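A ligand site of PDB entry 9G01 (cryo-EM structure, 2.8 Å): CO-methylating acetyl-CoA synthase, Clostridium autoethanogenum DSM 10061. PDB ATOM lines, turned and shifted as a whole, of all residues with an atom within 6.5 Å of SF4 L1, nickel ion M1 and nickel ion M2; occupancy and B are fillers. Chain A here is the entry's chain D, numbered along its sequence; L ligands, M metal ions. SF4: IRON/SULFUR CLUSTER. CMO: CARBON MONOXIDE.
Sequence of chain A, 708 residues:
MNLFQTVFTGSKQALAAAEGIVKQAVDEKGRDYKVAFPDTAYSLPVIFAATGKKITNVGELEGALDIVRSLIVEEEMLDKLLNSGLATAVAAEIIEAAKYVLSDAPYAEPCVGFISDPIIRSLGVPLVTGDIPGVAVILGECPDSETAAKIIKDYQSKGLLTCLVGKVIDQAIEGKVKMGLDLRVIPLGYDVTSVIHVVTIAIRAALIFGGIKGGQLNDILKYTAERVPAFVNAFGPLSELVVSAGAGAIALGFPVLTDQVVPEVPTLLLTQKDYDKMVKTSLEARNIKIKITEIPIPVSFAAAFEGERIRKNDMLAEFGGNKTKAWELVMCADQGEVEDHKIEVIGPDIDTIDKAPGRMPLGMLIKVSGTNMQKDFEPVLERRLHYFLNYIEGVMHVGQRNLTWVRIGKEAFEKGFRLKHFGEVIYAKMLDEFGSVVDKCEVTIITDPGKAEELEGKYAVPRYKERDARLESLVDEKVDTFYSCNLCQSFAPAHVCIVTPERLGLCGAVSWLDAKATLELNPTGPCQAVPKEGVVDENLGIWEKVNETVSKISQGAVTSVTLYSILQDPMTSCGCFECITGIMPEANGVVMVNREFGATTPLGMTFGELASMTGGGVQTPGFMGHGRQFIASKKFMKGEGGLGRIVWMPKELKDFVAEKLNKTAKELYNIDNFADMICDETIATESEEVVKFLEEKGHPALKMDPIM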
ATOM      1  N   GLY A 124      -8.487  -7.224  12.567  1.00  0.00           N
ATOM      2  CA  GLY A 124      -7.759  -7.157  11.317  1.00  0.00           C
ATOM      3  C   GLY A 124      -7.841  -8.436  10.513  1.00  0.00           C
ATOM      4  O   GLY A 124      -8.010  -8.410   9.296  1.00  0.00           O
ATOM      5  N   VAL A 125      -7.710  -9.588  11.174  1.00  0.00           N
ATOM      6  CA  VAL A 125      -7.802 -10.899  10.514  1.00  0.00           C
ATOM      7  C   VAL A 125      -9.182 -11.092   9.901  1.00  0.00           C
ATOM      8  O   VAL A 125      -9.296 -11.384   8.707  1.00  0.00           O
ATOM      9  CB  VAL A 125      -7.412 -12.034  11.450  1.00  0.00           C
ATOM     10  CG1 VAL A 125      -7.831 -13.372  10.860  1.00  0.00           C
ATOM     11  CG2 VAL A 125      -5.916 -12.017  11.680  1.00  0.00           C
ATOM     12  N   VAL A 128      -9.386  -9.498   6.648  1.00  0.00           N
ATOM     13  CA  VAL A 128      -8.617 -10.116   5.549  1.00  0.00           C
ATOM     14  C   VAL A 128      -9.226 -11.441   5.111  1.00  0.00           C
ATOM     15  O   VAL A 128      -9.241 -11.765   3.920  1.00  0.00           O
ATOM     16  CB  VAL A 128      -7.105 -10.268   5.862  1.00  0.00           C
ATOM     17  CG1 VAL A 128      -6.455  -8.910   6.034  1.00  0.00           C
ATOM     18  CG2 VAL A 128      -6.805 -11.182   7.035  1.00  0.00           C
ATOM     19  N   PHE A 209      -1.812  -1.806   8.980  1.00  0.00           N
ATOM     20  CA  PHE A 209      -1.675  -2.895   8.015  1.00  0.00           C
ATOM     21  C   PHE A 209      -1.019  -2.420   6.731  1.00  0.00           C
ATOM     22  O   PHE A 209      -0.211  -3.145   6.144  1.00  0.00           O
ATOM     23  CB  PHE A 209      -3.041  -3.509   7.715  1.00  0.00           C
ATOM     24  CG  PHE A 209      -3.783  -3.928   8.944  1.00  0.00           C
ATOM     25  CD1 PHE A 209      -3.329  -4.971   9.723  1.00  0.00           C
ATOM     26  CD2 PHE A 209      -4.944  -3.290   9.307  1.00  0.00           C
ATOM     27  CE1 PHE A 209      -4.019  -5.369  10.843  1.00  0.00           C
ATOM     28  CE2 PHE A 209      -5.644  -3.677  10.427  1.00  0.00           C
ATOM     29  CZ  PHE A 209      -5.171  -4.713  11.197  1.00  0.00           C
ATOM     30  N   CYS A 485       1.783 -18.140   3.084  1.00  0.00           N
ATOM     31  CA  CYS A 485       0.431 -17.609   3.143  1.00  0.00           C
ATOM     32  C   CYS A 485       0.488 -16.129   2.785  1.00  0.00           C
ATOM     33  O   CYS A 485       1.190 -15.361   3.451  1.00  0.00           O
ATOM     34  CB  CYS A 485      -0.155 -17.826   4.540  1.00  0.00           C
ATOM     35  SG  CYS A 485      -1.855 -17.265   4.711  1.00  0.00           S
ATOM     36  N   ASN A 486      -0.235 -15.734   1.728  1.00  0.00           N
ATOM     37  CA  ASN A 486      -0.358 -14.346   1.327  1.00  0.00           C
ATOM     38  C   ASN A 486      -1.778 -13.831   1.525  1.00  0.00           C
ATOM     39  O   ASN A 486      -2.216 -12.911   0.849  1.00  0.00           O
ATOM     40  CB  ASN A 486       0.093 -14.138  -0.119  1.00  0.00           C
ATOM     41  CG  ASN A 486      -0.792 -14.879  -1.129  1.00  0.00           C
ATOM     42  OD1 ASN A 486      -0.517 -16.023  -1.477  1.00  0.00           O
ATOM     43  ND2 ASN A 486      -1.864 -14.230  -1.587  1.00  0.00           N
ATOM     44  N   LEU A 487      -2.499 -14.431   2.484  1.00  0.00           N
ATOM     45  CA  LEU A 487      -3.876 -14.014   2.740  1.00  0.00           C
ATOM     46  C   LEU A 487      -3.919 -12.575   3.233  1.00  0.00           C
ATOM     47  O   LEU A 487      -4.805 -11.810   2.831  1.00  0.00           O
ATOM     48  CB  LEU A 487      -4.523 -14.963   3.758  1.00  0.00           C
ATOM     49  CG  LEU A 487      -6.013 -14.701   4.034  1.00  0.00           C
ATOM     50  CD1 LEU A 487      -6.860 -14.809   2.763  1.00  0.00           C
ATOM     51  CD2 LEU A 487      -6.509 -15.674   5.094  1.00  0.00           C
ATOM     52  N   CYS A 488      -2.985 -12.194   4.085  1.00  0.00           N
ATOM     53  CA  CYS A 488      -2.965 -10.844   4.655  1.00  0.00           C
ATOM     54  C   CYS A 488      -2.500  -9.785   3.680  1.00  0.00           C
ATOM     55  O   CYS A 488      -2.335  -8.635   4.086  1.00  0.00           O
ATOM     56  CB  CYS A 488      -2.068 -10.806   5.898  1.00  0.00           C
ATOM     57  SG  CYS A 488      -2.840 -11.472   7.394  1.00  0.00           S
ATOM     58  N   GLN A 489      -2.289 -10.109   2.404  1.00  0.00           N
ATOM     59  CA  GLN A 489      -1.902  -9.114   1.414  1.00  0.00           C
ATOM     60  C   GLN A 489      -3.049  -8.206   1.007  1.00  0.00           C
ATOM     61  O   GLN A 489      -2.802  -7.175   0.364  1.00  0.00           O
ATOM     62  CB  GLN A 489      -1.327  -9.776   0.172  1.00  0.00           C
ATOM     63  CG  GLN A 489       0.123 -10.228   0.338  1.00  0.00           C
ATOM     64  CD  GLN A 489       0.788 -10.569  -0.992  1.00  0.00           C
ATOM     65  OE1 GLN A 489       1.977 -10.867  -1.022  1.00  0.00           O
ATOM     66  NE2 GLN A 489       0.022 -10.526  -2.090  1.00  0.00           N
ATOM     67  N   ALA A 492      -1.924  -5.693   3.721  1.00  0.00           N
ATOM     68  CA  ALA A 492      -0.490  -5.468   3.770  1.00  0.00           C
ATOM     69  C   ALA A 492       0.142  -6.017   2.492  1.00  0.00           C
ATOM     70  O   ALA A 492       0.564  -7.183   2.448  1.00  0.00           O
ATOM     71  CB  ALA A 492       0.130  -6.130   5.006  1.00  0.00           C
ATOM     72  N   HIS A 495       3.615  -7.964   2.682  1.00  0.00           N
ATOM     73  CA  HIS A 495       3.799  -8.974   3.716  1.00  0.00           C
ATOM     74  C   HIS A 495       3.502 -10.364   3.171  1.00  0.00           C
ATOM     75  O   HIS A 495       2.429 -10.599   2.598  1.00  0.00           O
ATOM     76  CB  HIS A 495       2.886  -8.690   4.908  1.00  0.00           C
ATOM     77  CG  HIS A 495       2.784  -9.843   5.858  1.00  0.00           C
ATOM     78  ND1 HIS A 495       3.861 -10.344   6.544  1.00  0.00           N
ATOM     79  CD2 HIS A 495       1.726 -10.614   6.220  1.00  0.00           C
ATOM     80  CE1 HIS A 495       3.492 -11.367   7.286  1.00  0.00           C
ATOM     81  NE2 HIS A 495       2.184 -11.548   7.115  1.00  0.00           N
ATOM     82  N   VAL A 496       4.453 -11.278   3.349  1.00  0.00           N
ATOM     83  CA  VAL A 496       4.313 -12.698   2.994  1.00  0.00           C
ATOM     84  C   VAL A 496       4.759 -13.531   4.183  1.00  0.00           C
ATOM     85  O   VAL A 496       5.868 -13.339   4.699  1.00  0.00           O
ATOM     86  CB  VAL A 496       5.133 -13.050   1.740  1.00  0.00           C
ATOM     87  CG1 VAL A 496       4.848 -14.498   1.316  1.00  0.00           C
ATOM     88  CG2 VAL A 496       4.825 -12.096   0.601  1.00  0.00           C
ATOM     89  N   CYS A 497       3.915 -14.462   4.617  1.00  0.00           N
ATOM     90  CA  CYS A 497       4.264 -15.395   5.681  1.00  0.00           C
ATOM     91  C   CYS A 497       4.888 -16.654   5.105  1.00  0.00           C
ATOM     92  O   CYS A 497       4.619 -17.024   3.958  1.00  0.00           O
ATOM     93  CB  CYS A 497       3.029 -15.787   6.499  1.00  0.00           C
ATOM     94  SG  CYS A 497       2.603 -14.607   7.790  1.00  0.00           S
ATOM     95  N   ILE A 498       5.736 -17.296   5.895  1.00  0.00           N
ATOM     96  CA  ILE A 498       6.338 -18.580   5.547  1.00  0.00           C
ATOM     97  C   ILE A 498       6.102 -19.494   6.738  1.00  0.00           C
ATOM     98  O   ILE A 498       6.861 -19.455   7.713  1.00  0.00           O
ATOM     99  CB  ILE A 498       7.832 -18.457   5.221  1.00  0.00           C
ATOM    100  CG1 ILE A 498       8.071 -17.406   4.124  1.00  0.00           C
ATOM    101  CG2 ILE A 498       8.394 -19.825   4.787  1.00  0.00           C
ATOM    102  CD1 ILE A 498       7.493 -17.793   2.755  1.00  0.00           C
ATOM    103  N   VAL A 499       5.051 -20.300   6.682  1.00  0.00           N
ATOM    104  CA  VAL A 499       4.732 -21.193   7.792  1.00  0.00           C
ATOM    105  C   VAL A 499       5.611 -22.423   7.703  1.00  0.00           C
ATOM    106  O   VAL A 499       5.650 -23.108   6.678  1.00  0.00           O
ATOM    107  CB  VAL A 499       3.231 -21.560   7.795  1.00  0.00           C
ATOM    108  CG1 VAL A 499       2.397 -20.370   8.238  1.00  0.00           C
ATOM    109  CG2 VAL A 499       2.773 -22.028   6.451  1.00  0.00           C
ATOM    110  N   LEU A 504       4.667 -21.167  12.998  1.00  0.00           N
ATOM    111  CA  LEU A 504       3.360 -21.029  12.375  1.00  0.00           C
ATOM    112  C   LEU A 504       3.124 -19.582  11.957  1.00  0.00           C
ATOM    113  O   LEU A 504       3.956 -18.703  12.172  1.00  0.00           O
ATOM    114  CB  LEU A 504       2.259 -21.520  13.323  1.00  0.00           C
ATOM    115  CG  LEU A 504       1.832 -20.601  14.476  1.00  0.00           C
ATOM    116  CD1 LEU A 504       0.523 -21.127  15.069  1.00  0.00           C
ATOM    117  CD2 LEU A 504       2.900 -20.497  15.564  1.00  0.00           C
ATOM    118  N   GLY A 505       1.962 -19.317  11.356  1.00  0.00           N
ATOM    119  CA  GLY A 505       1.633 -17.959  10.961  1.00  0.00           C
ATOM    120  C   GLY A 505       1.531 -17.044  12.165  1.00  0.00           C
ATOM    121  O   GLY A 505       1.059 -17.430  13.229  1.00  0.00           O
ATOM    122  N   LEU A 506       1.985 -15.806  11.984  1.00  0.00           N
ATOM    123  CA  LEU A 506       2.002 -14.865  13.102  1.00  0.00           C
ATOM    124  C   LEU A 506       0.600 -14.543  13.598  1.00  0.00           C
ATOM    125  O   LEU A 506       0.441 -14.169  14.770  1.00  0.00           O
ATOM    126  CB  LEU A 506       2.760 -13.589  12.718  1.00  0.00           C
ATOM    127  CG  LEU A 506       2.268 -12.798  11.504  1.00  0.00           C
ATOM    128  CD1 LEU A 506       1.484 -11.561  11.928  1.00  0.00           C
ATOM    129  CD2 LEU A 506       3.455 -12.403  10.653  1.00  0.00           C
ATOM    130  N   CYS A 507      -0.414 -14.708  12.757  1.00  0.00           N
ATOM    131  CA  CYS A 507      -1.791 -14.547  13.222  1.00  0.00           C
ATOM    132  C   CYS A 507      -2.200 -15.650  14.196  1.00  0.00           C
ATOM    133  O   CYS A 507      -3.128 -15.450  14.980  1.00  0.00           O
ATOM    134  CB  CYS A 507      -2.754 -14.494  12.036  1.00  0.00           C
ATOM    135  SG  CYS A 507      -2.826 -16.043  11.122  1.00  0.00           S
ATOM    136  N   GLY A 508      -1.540 -16.806  14.138  1.00  0.00           N
ATOM    137  CA  GLY A 508      -1.848 -17.909  15.021  1.00  0.00           C
ATOM    138  C   GLY A 508      -2.925 -18.849  14.518  1.00  0.00           C
ATOM    139  O   GLY A 508      -3.146 -19.895  15.132  1.00  0.00           O
ATOM    140  N   ALA A 509      -3.597 -18.512  13.411  1.00  0.00           N
ATOM    141  CA  ALA A 509      -4.664 -19.334  12.881  1.00  0.00           C
ATOM    142  C   ALA A 509      -4.227 -20.206  11.713  1.00  0.00           C
ATOM    143  O   ALA A 509      -5.007 -21.060  11.274  1.00  0.00           O
ATOM    144  CB  ALA A 509      -5.858 -18.451  12.450  1.00  0.00           C
ATOM    145  N   VAL A 510      -3.016 -20.007  11.194  1.00  0.00           N
ATOM    146  CA  VAL A 510      -2.501 -20.795  10.081  1.00  0.00           C
ATOM    147  C   VAL A 510      -1.257 -21.535  10.590  1.00  0.00           C
ATOM    148  O   VAL A 510      -0.315 -20.907  11.077  1.00  0.00           O
ATOM    149  CB  VAL A 510      -2.158 -19.925   8.865  1.00  0.00           C
ATOM    150  CG1 VAL A 510      -1.667 -20.794   7.714  1.00  0.00           C
ATOM    151  CG2 VAL A 510      -3.366 -19.113   8.437  1.00  0.00           C
ATOM    152  N   PRO A 526      -4.482 -18.738  -0.692  1.00  0.00           N
ATOM    153  CA  PRO A 526      -3.282 -18.032  -0.201  1.00  0.00           C
ATOM    154  C   PRO A 526      -2.103 -18.928   0.104  1.00  0.00           C
ATOM    155  O   PRO A 526      -0.955 -18.493  -0.044  1.00  0.00           O
ATOM    156  CB  PRO A 526      -3.796 -17.303   1.055  1.00  0.00           C
ATOM    157  CG  PRO A 526      -4.991 -18.138   1.520  1.00  0.00           C
ATOM    158  CD  PRO A 526      -5.628 -18.629   0.236  1.00  0.00           C
ATOM    159  N   CYS A 527      -2.333 -20.173   0.527  1.00  0.00           N
ATOM    160  CA  CYS A 527      -1.244 -21.067   0.916  1.00  0.00           C
ATOM    161  C   CYS A 527      -0.725 -21.811  -0.298  1.00  0.00           C
ATOM    162  O   CYS A 527      -1.483 -22.495  -0.992  1.00  0.00           O
ATOM    163  CB  CYS A 527      -1.733 -22.062   1.983  1.00  0.00           C
ATOM    164  SG  CYS A 527      -2.237 -21.271   3.520  1.00  0.00           S
ATOM    165  N   SER A 573       5.869  -8.732   9.440  1.00  0.00           N
ATOM    166  CA  SER A 573       4.561  -8.907  10.035  1.00  0.00           C
ATOM    167  C   SER A 573       3.669  -7.796   9.534  1.00  0.00           C
ATOM    168  O   SER A 573       4.153  -6.785   9.012  1.00  0.00           O
ATOM    169  CB  SER A 573       4.608  -8.860  11.582  1.00  0.00           C
ATOM    170  OG  SER A 573       5.529  -9.809  12.118  1.00  0.00           O
ATOM    171  N   CYS A 574       2.345  -7.959   9.661  1.00  0.00           N
ATOM    172  CA  CYS A 574       1.417  -6.988   9.118  1.00  0.00           C
ATOM    173  C   CYS A 574       0.733  -6.252  10.264  1.00  0.00           C
ATOM    174  O   CYS A 574       1.031  -5.070  10.491  1.00  0.00           O
ATOM    175  CB  CYS A 574       0.401  -7.698   8.213  1.00  0.00           C
ATOM    176  SG  CYS A 574      -0.098  -9.289   8.899  1.00  0.00           S
ATOM    177  N   GLY A 575      -0.194  -6.877  10.973  1.00  0.00           N
ATOM    178  CA  GLY A 575      -0.759  -6.233  12.151  1.00  0.00           C
ATOM    179  C   GLY A 575      -1.391  -7.187  13.140  1.00  0.00           C
ATOM    180  O   GLY A 575      -1.956  -6.765  14.149  1.00  0.00           O
ATOM    181  N   CYS A 576      -1.290  -8.488  12.873  1.00  0.00           N
ATOM    182  CA  CYS A 576      -2.145  -9.490  13.493  1.00  0.00           C
ATOM    183  C   CYS A 576      -1.410 -10.436  14.429  1.00  0.00           C
ATOM    184  O   CYS A 576      -2.003 -11.393  14.927  1.00  0.00           O
ATOM    185  CB  CYS A 576      -2.859 -10.291  12.397  1.00  0.00           C
ATOM    186  SG  CYS A 576      -1.715 -10.843  11.103  1.00  0.00           S
ATOM    187  N   PHE A 577      -0.133 -10.169  14.698  1.00  0.00           N
ATOM    188  CA  PHE A 577       0.639 -11.059  15.559  1.00  0.00           C
ATOM    189  C   PHE A 577       0.061 -11.094  16.963  1.00  0.00           C
ATOM    190  O   PHE A 577      -0.290 -10.053  17.524  1.00  0.00           O
ATOM    191  CB  PHE A 577       2.108 -10.626  15.583  1.00  0.00           C
ATOM    192  CG  PHE A 577       2.306  -9.145  15.564  1.00  0.00           C
ATOM    193  CD1 PHE A 577       2.273  -8.408  16.735  1.00  0.00           C
ATOM    194  CD2 PHE A 577       2.497  -8.478  14.350  1.00  0.00           C
ATOM    195  CE1 PHE A 577       2.443  -7.013  16.721  1.00  0.00           C
ATOM    196  CE2 PHE A 577       2.668  -7.101  14.308  1.00  0.00           C
ATOM    197  CZ  PHE A 577       2.643  -6.357  15.493  1.00  0.00           C
HETATM  198 FE1  SF4 L   1      -1.874 -15.894   6.530  1.00  0.00          FE
HETATM  199 FE2  SF4 L   1       0.351 -14.725   7.601  1.00  0.00          FE
HETATM  200 FE3  SF4 L   1      -1.669 -15.561   9.234  1.00  0.00          FE
HETATM  201 FE4  SF4 L   1      -2.031 -13.386   7.612  1.00  0.00          FE
HETATM  202  S1  SF4 L   1      -0.559 -13.572   9.340  1.00  0.00           S
HETATM  203  S2  SF4 L   1      -3.489 -15.108   7.942  1.00  0.00           S
HETATM  204  S3  SF4 L   1      -0.830 -14.010   5.779  1.00  0.00           S
HETATM  205  S4  SF4 L   1      -0.362 -16.872   7.918  1.00  0.00           S
HETATM  206  C   CMO L   2      -3.647  -8.834   8.743  1.00  0.00           C
HETATM  207  O   CMO L   2      -4.583  -8.033   8.604  1.00  0.00           O
HETATM  208 NI    NI M   1      -2.409  -9.876   8.930  1.00  0.00          NI
HETATM  209 NI    NI M   2      -0.803  -8.784  10.991  1.00  0.00          NI
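Residues that only touch SF4 L1: Leu 506 (3.6 Å), Val 510 (3.7 Å), His 495 (3.7 Å) and Gly 505 (3.8 Å).
Hydrophobic or aromatic side chains within 4 Å of SF4 L1: Leu 487, Leu 506 and Val 510.
Within 4 Å of SF4 L1: Cys 485, Leu 487, Cys 488, His 495, Cys 497, Gly 505, Leu 506, Cys 507, Val 510 and Cys 576.
Nickel ion M2 is bound by N of Cys 576, N of Gly 575, SG of Cys 576 and SG of Cys 574.
SG of Cys 488 is bound to nickel ion M1.
Nickel ion M1 is bound by SG of Cys 574, 2.4 Å away.
SG of Cys 576 binds nickel ion M1, at 2.5 Å.
N of Cys 488 sits close to S3 of SF4 L1, at 3.3 Å.
SG of Cys 488 is bound to FE4 of SF4 L1.
An iron atom (FE2) of SF4 L1 is bound by the side-chain sulfur (SG) of Cys 497.
A sulfur (S1) of SF4 L1 sits close to the backbone NH of Cys 507 (3.6 Å).
SG of Cys 507 binds FE3 of SF4 L1, at 2.3 Å.
An iron atom (FE1) of SF4 L1 is bound by the side-chain sulfur of Cys 485, at 2.3 Å.
A sulfur (S3) of SF4 L1 lies close to the backbone NH (N) of Leu 487 (3.7 Å).
The backbone NH of Cys 497 is in hydrogen-bond range of the backbone carbonyl oxygen of Cys 485 (3.1 Å).
The side-chain sulfur of Cys 497 sits close to a ring nitrogen (NE2) of His 495.
SG of Cys 574 sits close to NE2 of His 495.
SG of Cys 507 lies close to N of Ala 509, at 3.5 Å.
SG of Cys 485 sits close to N of Leu 487 (3.7 Å).
O of Val 510 sits at hydrogen-bond distance from N of Gly 505, 2.8 Å away.
Merely in contact with nickel ion M2: Leu 506 (3.7 Å).
Four residues have an atom within 4 Å of nickel ion M2: Leu 506, Cys 574, Gly 575 and Cys 576.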
